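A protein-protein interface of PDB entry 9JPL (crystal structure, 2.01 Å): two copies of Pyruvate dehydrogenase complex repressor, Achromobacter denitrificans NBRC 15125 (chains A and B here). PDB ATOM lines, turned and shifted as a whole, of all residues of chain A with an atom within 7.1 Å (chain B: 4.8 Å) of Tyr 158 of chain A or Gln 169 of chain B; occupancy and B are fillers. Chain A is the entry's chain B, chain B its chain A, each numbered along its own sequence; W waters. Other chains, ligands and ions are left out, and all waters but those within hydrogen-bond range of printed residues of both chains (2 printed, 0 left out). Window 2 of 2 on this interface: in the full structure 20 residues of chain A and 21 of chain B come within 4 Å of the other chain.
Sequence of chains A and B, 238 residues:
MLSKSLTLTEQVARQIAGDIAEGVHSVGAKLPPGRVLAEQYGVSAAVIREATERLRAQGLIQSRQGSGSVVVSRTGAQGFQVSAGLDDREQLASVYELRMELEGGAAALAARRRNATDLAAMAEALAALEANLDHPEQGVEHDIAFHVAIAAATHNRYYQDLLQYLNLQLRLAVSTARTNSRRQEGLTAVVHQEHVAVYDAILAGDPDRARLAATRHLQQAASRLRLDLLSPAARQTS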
ATOM      1  N   THR A 154      29.621 -12.013 -23.112  1.00  0.00           N
ATOM      2  CA  THR A 154      30.023 -11.429 -24.391  1.00  0.00           C
ATOM      3  C   THR A 154      31.302 -10.614 -24.270  1.00  0.00           C
ATOM      4  O   THR A 154      31.962 -10.367 -25.286  1.00  0.00           O
ATOM      5  CB  THR A 154      28.936 -10.516 -24.946  1.00  0.00           C
ATOM      6  OG1 THR A 154      28.773  -9.393 -24.069  1.00  0.00           O
ATOM      7  CG2 THR A 154      27.598 -11.270 -25.105  1.00  0.00           C
ATOM      8  N   HIS A 155      31.639 -10.167 -23.058  1.00  0.00           N
ATOM      9  CA  HIS A 155      32.724  -9.214 -22.833  1.00  0.00           C
ATOM     10  C   HIS A 155      32.518  -7.945 -23.645  1.00  0.00           C
ATOM     11  O   HIS A 155      33.469  -7.296 -24.082  1.00  0.00           O
ATOM     12  CB  HIS A 155      34.079  -9.865 -23.114  1.00  0.00           C
ATOM     13  CG  HIS A 155      34.452 -10.853 -22.062  1.00  0.00           C
ATOM     14  ND1 HIS A 155      35.085 -10.484 -20.892  1.00  0.00           N
ATOM     15  CD2 HIS A 155      34.194 -12.177 -21.953  1.00  0.00           C
ATOM     16  CE1 HIS A 155      35.244 -11.551 -20.129  1.00  0.00           C
ATOM     17  NE2 HIS A 155      34.710 -12.591 -20.748  1.00  0.00           N
ATOM     18  N   ASN A 156      31.252  -7.582 -23.825  1.00  0.00           N
ATOM     19  CA  ASN A 156      30.866  -6.358 -24.504  1.00  0.00           C
ATOM     20  C   ASN A 156      30.051  -5.549 -23.506  1.00  0.00           C
ATOM     21  O   ASN A 156      28.925  -5.927 -23.167  1.00  0.00           O
ATOM     22  CB  ASN A 156      30.090  -6.680 -25.784  1.00  0.00           C
ATOM     23  CG  ASN A 156      29.650  -5.448 -26.524  1.00  0.00           C
ATOM     24  OD1 ASN A 156      29.180  -4.481 -25.929  1.00  0.00           O
ATOM     25  ND2 ASN A 156      29.764  -5.487 -27.841  1.00  0.00           N
ATOM     26  N   ARG A 157      30.622  -4.433 -23.048  1.00  0.00           N
ATOM     27  CA  ARG A 157      29.998  -3.636 -22.000  1.00  0.00           C
ATOM     28  C   ARG A 157      28.615  -3.141 -22.413  1.00  0.00           C
ATOM     29  O   ARG A 157      27.741  -2.968 -21.559  1.00  0.00           O
ATOM     30  CB  ARG A 157      30.891  -2.445 -21.642  1.00  0.00           C
ATOM     31  CG  ARG A 157      30.998  -1.398 -22.774  1.00  0.00           C
ATOM     32  CD  ARG A 157      31.914  -0.201 -22.435  1.00  0.00           C
ATOM     33  NE  ARG A 157      33.342  -0.490 -22.621  1.00  0.00           N
ATOM     34  CZ  ARG A 157      33.963  -0.525 -23.801  1.00  0.00           C
ATOM     35  NH1 ARG A 157      35.260  -0.798 -23.863  1.00  0.00           N
ATOM     36  NH2 ARG A 157      33.290  -0.295 -24.922  1.00  0.00           N
ATOM     37  N   TYR A 158      28.396  -2.905 -23.706  1.00  0.00           N
ATOM     38  CA  TYR A 158      27.123  -2.325 -24.114  1.00  0.00           C
ATOM     39  C   TYR A 158      25.995  -3.337 -24.073  1.00  0.00           C
ATOM     40  O   TYR A 158      24.863  -2.964 -23.755  1.00  0.00           O
ATOM     41  CB  TYR A 158      27.269  -1.683 -25.488  1.00  0.00           C
ATOM     42  CG  TYR A 158      28.277  -0.564 -25.412  1.00  0.00           C
ATOM     43  CD1 TYR A 158      28.057   0.529 -24.588  1.00  0.00           C
ATOM     44  CD2 TYR A 158      29.469  -0.630 -26.107  1.00  0.00           C
ATOM     45  CE1 TYR A 158      28.982   1.547 -24.492  1.00  0.00           C
ATOM     46  CE2 TYR A 158      30.403   0.376 -26.017  1.00  0.00           C
ATOM     47  CZ  TYR A 158      30.160   1.464 -25.210  1.00  0.00           C
ATOM     48  OH  TYR A 158      31.107   2.467 -25.113  1.00  0.00           O
ATOM     49  N   TYR A 159      26.277  -4.613 -24.350  1.00  0.00           N
ATOM     50  CA  TYR A 159      25.257  -5.640 -24.152  1.00  0.00           C
ATOM     51  C   TYR A 159      24.818  -5.687 -22.708  1.00  0.00           C
ATOM     52  O   TYR A 159      23.621  -5.768 -22.410  1.00  0.00           O
ATOM     53  CB  TYR A 159      25.784  -7.013 -24.536  1.00  0.00           C
ATOM     54  CG  TYR A 159      25.495  -7.417 -25.936  1.00  0.00           C
ATOM     55  CD1 TYR A 159      24.266  -7.968 -26.298  1.00  0.00           C
ATOM     56  CD2 TYR A 159      26.463  -7.254 -26.897  1.00  0.00           C
ATOM     57  CE1 TYR A 159      24.030  -8.343 -27.599  1.00  0.00           C
ATOM     58  CE2 TYR A 159      26.245  -7.615 -28.172  1.00  0.00           C
ATOM     59  CZ  TYR A 159      25.048  -8.159 -28.522  1.00  0.00           C
ATOM     60  OH  TYR A 159      24.920  -8.500 -29.821  1.00  0.00           O
ATOM     61  N   GLN A 160      25.786  -5.683 -21.790  1.00  0.00           N
ATOM     62  CA  GLN A 160      25.444  -5.739 -20.377  1.00  0.00           C
ATOM     63  C   GLN A 160      24.621  -4.530 -19.973  1.00  0.00           C
ATOM     64  O   GLN A 160      23.630  -4.661 -19.248  1.00  0.00           O
ATOM     65  CB  GLN A 160      26.710  -5.822 -19.530  1.00  0.00           C
ATOM     66  CG  GLN A 160      27.738  -6.793 -20.061  1.00  0.00           C
ATOM     67  CD  GLN A 160      28.886  -6.963 -19.076  1.00  0.00           C
ATOM     68  OE1 GLN A 160      28.665  -6.987 -17.861  1.00  0.00           O
ATOM     69  NE2 GLN A 160      30.111  -7.079 -19.591  1.00  0.00           N
ATOM     70  N   ASP A 161      25.020  -3.338 -20.427  1.00  0.00           N
ATOM     71  CA  ASP A 161      24.284  -2.147 -20.015  1.00  0.00           C
ATOM     72  C   ASP A 161      22.873  -2.130 -20.588  1.00  0.00           C
ATOM     73  O   ASP A 161      21.954  -1.627 -19.937  1.00  0.00           O
ATOM     74  CB  ASP A 161      25.045  -0.884 -20.405  1.00  0.00           C
ATOM     75  CG  ASP A 161      26.103  -0.514 -19.384  1.00  0.00           C
ATOM     76  OD1 ASP A 161      26.780  -1.430 -18.852  1.00  0.00           O
ATOM     77  OD2 ASP A 161      26.241   0.693 -19.088  1.00  0.00           O
ATOM     78  N   LEU A 162      22.673  -2.690 -21.785  1.00  0.00           N
ATOM     79  CA  LEU A 162      21.337  -2.728 -22.378  1.00  0.00           C
ATOM     80  C   LEU A 162      20.390  -3.626 -21.588  1.00  0.00           C
ATOM     81  O   LEU A 162      19.206  -3.294 -21.418  1.00  0.00           O
ATOM     82  CB  LEU A 162      21.429  -3.191 -23.827  1.00  0.00           C
ATOM     83  CG  LEU A 162      21.420  -2.072 -24.861  1.00  0.00           C
ATOM     84  CD1 LEU A 162      22.392  -0.984 -24.472  1.00  0.00           C
ATOM     85  CD2 LEU A 162      21.749  -2.649 -26.217  1.00  0.00           C
ATOM     86  N   LEU A 163      20.888  -4.773 -21.105  1.00  0.00           N
ATOM     87  CA  LEU A 163      20.044  -5.695 -20.348  1.00  0.00           C
ATOM     88  C   LEU A 163      19.723  -5.137 -18.976  1.00  0.00           C
ATOM     89  O   LEU A 163      18.626  -5.363 -18.448  1.00  0.00           O
ATOM     90  CB  LEU A 163      20.727  -7.054 -20.202  1.00  0.00           C
ATOM     91  CG  LEU A 163      20.196  -8.151 -21.111  1.00  0.00           C
ATOM     92  CD1 LEU A 163      20.644  -7.889 -22.535  1.00  0.00           C
ATOM     93  CD2 LEU A 163      20.659  -9.521 -20.619  1.00  0.00           C
ATOM     94  N   GLN A 164      20.670  -4.418 -18.374  1.00  0.00           N
ATOM     95  CA  GLN A 164      20.364  -3.733 -17.129  1.00  0.00           C
ATOM     96  C   GLN A 164      19.369  -2.601 -17.370  1.00  0.00           C
ATOM     97  O   GLN A 164      18.499  -2.338 -16.531  1.00  0.00           O
ATOM     98  CB  GLN A 164      21.647  -3.200 -16.493  1.00  0.00           C
ATOM     99  CG  GLN A 164      21.466  -2.817 -15.028  1.00  0.00           C
ATOM    100  CD  GLN A 164      22.103  -1.486 -14.682  1.00  0.00           C
ATOM    101  OE1 GLN A 164      21.640  -0.430 -15.125  1.00  0.00           O
ATOM    102  NE2 GLN A 164      23.161  -1.523 -13.867  1.00  0.00           N
ATOM    103  N   GLN B  91      36.451  -0.512 -28.134  1.00  0.00           N
ATOM    104  CA  GLN B  91      35.169   0.126 -27.883  1.00  0.00           C
ATOM    105  C   GLN B  91      34.357   0.254 -29.169  1.00  0.00           C
ATOM    106  O   GLN B  91      33.153  -0.026 -29.177  1.00  0.00           O
ATOM    107  CB  GLN B  91      35.383   1.495 -27.248  1.00  0.00           C
ATOM    108  CG  GLN B  91      34.073   2.271 -27.071  1.00  0.00           C
ATOM    109  CD  GLN B  91      34.264   3.635 -26.436  1.00  0.00           C
ATOM    110  OE1 GLN B  91      35.219   4.347 -26.750  1.00  0.00           O
ATOM    111  NE2 GLN B  91      33.347   4.012 -25.547  1.00  0.00           N
ATOM    112  N   SER B  94      33.040  -3.028 -30.167  1.00  0.00           N
ATOM    113  CA  SER B  94      31.906  -3.402 -29.326  1.00  0.00           C
ATOM    114  C   SER B  94      30.611  -2.725 -29.779  1.00  0.00           C
ATOM    115  O   SER B  94      29.531  -3.335 -29.737  1.00  0.00           O
ATOM    116  CB  SER B  94      32.221  -3.043 -27.878  1.00  0.00           C
ATOM    117  OG  SER B  94      33.022  -4.042 -27.291  1.00  0.00           O
ATOM    118  N   VAL B  95      30.695  -1.460 -30.197  1.00  0.00           N
ATOM    119  CA  VAL B  95      29.510  -0.747 -30.675  1.00  0.00           C
ATOM    120  C   VAL B  95      29.010  -1.368 -31.970  1.00  0.00           C
ATOM    121  O   VAL B  95      27.800  -1.602 -32.147  1.00  0.00           O
ATOM    122  CB  VAL B  95      29.818   0.756 -30.850  1.00  0.00           C
ATOM    123  CG1 VAL B  95      28.624   1.490 -31.514  1.00  0.00           C
ATOM    124  CG2 VAL B  95      30.157   1.408 -29.504  1.00  0.00           C
ATOM    125  N   LEU B  98      27.264  -4.794 -31.397  1.00  0.00           N
ATOM    126  CA  LEU B  98      25.917  -4.640 -30.858  1.00  0.00           C
ATOM    127  C   LEU B  98      24.955  -4.094 -31.913  1.00  0.00           C
ATOM    128  O   LEU B  98      23.812  -4.557 -32.018  1.00  0.00           O
ATOM    129  CB  LEU B  98      25.968  -3.732 -29.627  1.00  0.00           C
ATOM    130  CG  LEU B  98      24.622  -3.275 -29.064  1.00  0.00           C
ATOM    131  CD1 LEU B  98      23.784  -4.456 -28.555  1.00  0.00           C
ATOM    132  CD2 LEU B  98      24.850  -2.239 -27.968  1.00  0.00           C
ATOM    133  N   TYR B 165      18.940   5.661 -26.329  1.00  0.00           N
ATOM    134  CA  TYR B 165      19.828   5.396 -25.209  1.00  0.00           C
ATOM    135  C   TYR B 165      21.288   5.307 -25.653  1.00  0.00           C
ATOM    136  O   TYR B 165      22.189   5.699 -24.910  1.00  0.00           O
ATOM    137  CB  TYR B 165      19.379   4.097 -24.523  1.00  0.00           C
ATOM    138  CG  TYR B 165      20.181   3.739 -23.286  1.00  0.00           C
ATOM    139  CD1 TYR B 165      20.028   4.453 -22.105  1.00  0.00           C
ATOM    140  CD2 TYR B 165      21.079   2.681 -23.303  1.00  0.00           C
ATOM    141  CE1 TYR B 165      20.759   4.130 -20.976  1.00  0.00           C
ATOM    142  CE2 TYR B 165      21.818   2.350 -22.182  1.00  0.00           C
ATOM    143  CZ  TYR B 165      21.656   3.079 -21.021  1.00  0.00           C
ATOM    144  OH  TYR B 165      22.389   2.754 -19.904  1.00  0.00           O
ATOM    145  N   LEU B 166      21.539   4.808 -26.864  1.00  0.00           N
ATOM    146  CA  LEU B 166      22.886   4.631 -27.394  1.00  0.00           C
ATOM    147  C   LEU B 166      23.338   5.800 -28.256  1.00  0.00           C
ATOM    148  O   LEU B 166      24.262   5.641 -29.056  1.00  0.00           O
ATOM    149  CB  LEU B 166      22.958   3.336 -28.211  1.00  0.00           C
ATOM    150  CG  LEU B 166      22.744   2.026 -27.447  1.00  0.00           C
ATOM    151  CD1 LEU B 166      22.490   0.870 -28.417  1.00  0.00           C
ATOM    152  CD2 LEU B 166      23.940   1.734 -26.533  1.00  0.00           C
ATOM    153  N   ASN B 167      22.706   6.968 -28.129  1.00  0.00           N
ATOM    154  CA  ASN B 167      23.011   8.049 -29.062  1.00  0.00           C
ATOM    155  C   ASN B 167      24.478   8.479 -28.986  1.00  0.00           C
ATOM    156  O   ASN B 167      25.079   8.804 -30.015  1.00  0.00           O
ATOM    157  CB  ASN B 167      22.086   9.240 -28.811  1.00  0.00           C
ATOM    158  CG  ASN B 167      22.294  10.362 -29.819  1.00  0.00           C
ATOM    159  OD1 ASN B 167      22.860  11.408 -29.494  1.00  0.00           O
ATOM    160  ND2 ASN B 167      21.825  10.150 -31.049  1.00  0.00           N
ATOM    161  N   LEU B 168      25.089   8.451 -27.802  1.00  0.00           N
ATOM    162  CA  LEU B 168      26.494   8.854 -27.737  1.00  0.00           C
ATOM    163  C   LEU B 168      27.401   7.812 -28.384  1.00  0.00           C
ATOM    164  O   LEU B 168      28.397   8.164 -29.017  1.00  0.00           O
ATOM    165  CB  LEU B 168      26.922   9.099 -26.297  1.00  0.00           C
ATOM    166  CG  LEU B 168      26.129  10.174 -25.576  1.00  0.00           C
ATOM    167  CD1 LEU B 168      26.623  10.293 -24.136  1.00  0.00           C
ATOM    168  CD2 LEU B 168      26.230  11.507 -26.326  1.00  0.00           C
ATOM    169  N   GLN B 169      27.087   6.530 -28.213  1.00  0.00           N
ATOM    170  CA  GLN B 169      27.895   5.491 -28.840  1.00  0.00           C
ATOM    171  C   GLN B 169      27.731   5.523 -30.352  1.00  0.00           C
ATOM    172  O   GLN B 169      28.700   5.324 -31.087  1.00  0.00           O
ATOM    173  CB  GLN B 169      27.513   4.109 -28.304  1.00  0.00           C
ATOM    174  CG  GLN B 169      28.069   3.790 -26.942  1.00  0.00           C
ATOM    175  CD  GLN B 169      27.417   4.620 -25.858  1.00  0.00           C
ATOM    176  OE1 GLN B 169      26.189   4.717 -25.792  1.00  0.00           O
ATOM    177  NE2 GLN B 169      28.230   5.223 -25.005  1.00  0.00           N
ATOM    178  N   LEU B 170      26.506   5.765 -30.830  1.00  0.00           N
ATOM    179  CA  LEU B 170      26.270   5.888 -32.263  1.00  0.00           C
ATOM    180  C   LEU B 170      27.071   7.036 -32.839  1.00  0.00           C
ATOM    181  O   LEU B 170      27.705   6.898 -33.888  1.00  0.00           O
ATOM    182  CB  LEU B 170      24.774   6.099 -32.540  1.00  0.00           C
ATOM    183  CG  LEU B 170      23.922   4.850 -32.411  1.00  0.00           C
ATOM    184  CD1 LEU B 170      22.443   5.190 -32.478  1.00  0.00           C
ATOM    185  CD2 LEU B 170      24.287   3.914 -33.538  1.00  0.00           C
ATOM    186  N   ARG B 171      27.062   8.185 -32.157  1.00  0.00           N
ATOM    187  CA  ARG B 171      27.751   9.342 -32.704  1.00  0.00           C
ATOM    188  C   ARG B 171      29.249   9.092 -32.739  1.00  0.00           C
ATOM    189  O   ARG B 171      29.932   9.485 -33.690  1.00  0.00           O
ATOM    190  CB  ARG B 171      27.414  10.600 -31.896  1.00  0.00           C
ATOM    191  CG  ARG B 171      27.999  11.898 -32.514  1.00  0.00           C
ATOM    192  CD  ARG B 171      27.517  13.188 -31.799  1.00  0.00           C
ATOM    193  NE  ARG B 171      26.076  13.384 -31.981  1.00  0.00           N
ATOM    194  CZ  ARG B 171      25.162  13.082 -31.060  1.00  0.00           C
ATOM    195  NH1 ARG B 171      25.554  12.579 -29.888  1.00  0.00           N
ATOM    196  NH2 ARG B 171      23.860  13.274 -31.309  1.00  0.00           N
ATOM    197  N   LEU B 172      29.763   8.401 -31.719  1.00  0.00           N
ATOM    198  CA  LEU B 172      31.170   8.014 -31.698  1.00  0.00           C
ATOM    199  C   LEU B 172      31.517   7.122 -32.888  1.00  0.00           C
ATOM    200  O   LEU B 172      32.491   7.375 -33.615  1.00  0.00           O
ATOM    201  CB  LEU B 172      31.473   7.315 -30.367  1.00  0.00           C
ATOM    202  CG  LEU B 172      32.924   7.023 -29.961  1.00  0.00           C
ATOM    203  CD1 LEU B 172      33.369   5.709 -30.529  1.00  0.00           C
ATOM    204  CD2 LEU B 172      33.855   8.136 -30.398  1.00  0.00           C
ATOM    205  N   ALA B 173      30.746   6.055 -33.087  1.00  0.00           N
ATOM    206  CA  ALA B 173      31.024   5.144 -34.188  1.00  0.00           C
ATOM    207  C   ALA B 173      30.850   5.845 -35.532  1.00  0.00           C
ATOM    208  O   ALA B 173      31.721   5.758 -36.408  1.00  0.00           O
ATOM    209  CB  ALA B 173      30.103   3.932 -34.107  1.00  0.00           C
HETATM  210  O   HOH W   1      22.083   0.403 -17.978  1.00  0.00           O
HETATM  211  O   HOH W   2      33.149  -3.738 -24.313  1.00  0.00           O
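No position is printed for both chains.
Of the 13 printed residues of chain B, 6 touch a printed residue of chain A.
Hydrophobic or aromatic side chains of chain B within 4 Å of the printed part of chain A: Val 95, Leu 98 and Leu 166.
Of the 11 printed residues of chain A, 5 touch a printed residue of chain B.
Printed residues of chain A that touch a printed residue of chain B: Asn 156, Arg 157, Tyr 158, Tyr 159 and Leu 162.
Hydrophobic or aromatic side chains of chain A that line the printed part of chain B: Tyr 158, Tyr 159 and Leu 162.
Among the printed residues, no Asp or Glu carboxylate lies within 4 Å of a Lys or Arg side-chain nitrogen of the other chain.
Among the printed residues, merely in contact across the chains: Arg 157 of chain A with Gln 91 of chain B, Tyr 158 of chain A with Val 95 of chain B, Tyr 158 of chain A with Leu 98 of chain B, Tyr 158 of chain A with Gln 169 of chain B, Tyr 159 of chain A with Leu 98 of chain B, Leu 162 of chain A with Leu 98 of chain B and Leu 162 of chain A with Leu 166 of chain B.
Water W1 lies within hydrogen-bond range of O of Asp 161 of chain A (2.8 Å), OE1 of Gln 164 of chain A (3.0 Å) and OH of Tyr 165 of chain B (3.1 Å).
Water W2 lies within hydrogen-bond range of N of Arg 157 of chain A (2.9 Å) and OG of Ser 94 of chain B (3.0 Å).
OG1 of Thr 154 of chain A lies close to N of Asn 156 of chain A (3.1 Å).
OD1 of Asn 156 of chain A lies within hydrogen-bond range of N of Tyr 158 of chain A, at 2.8 Å.
N of Tyr 159 of chain A sits at hydrogen-bond distance from OD1 of Asn 156 of chain A (3.3 Å).
Printed residues of chain B within 4 Å of Asn 156 of chain A: Ser 94 (2.9 Å).
Of the printed residues of chain B, Arg 157 of chain A touches Gln 91.
Tyr 158 of chain A touches four residues of chain B.
Of the printed residues of chain A, Leu 166 of chain B touches Leu 162 (3.7 Å).
Gln 169 of chain B touches just one residue of chain A: Tyr 158.
The nearest residue of chain A that does not touch Gln 169 of chain B is Arg 157 of chain A (6.9 Å).
The side-chain hydroxyl (OH) of Tyr 158 of chain A lies within hydrogen-bond range of the side-chain amide nitrogen (NE2) of Gln 91 of chain B (2.8 Å).
The backbone carbonyl oxygen (O) of Ser 94 of chain B sits at hydrogen-bond distance from the side-chain amide nitrogen (ND2) of Asn 156 of chain A, at 2.9 Å.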
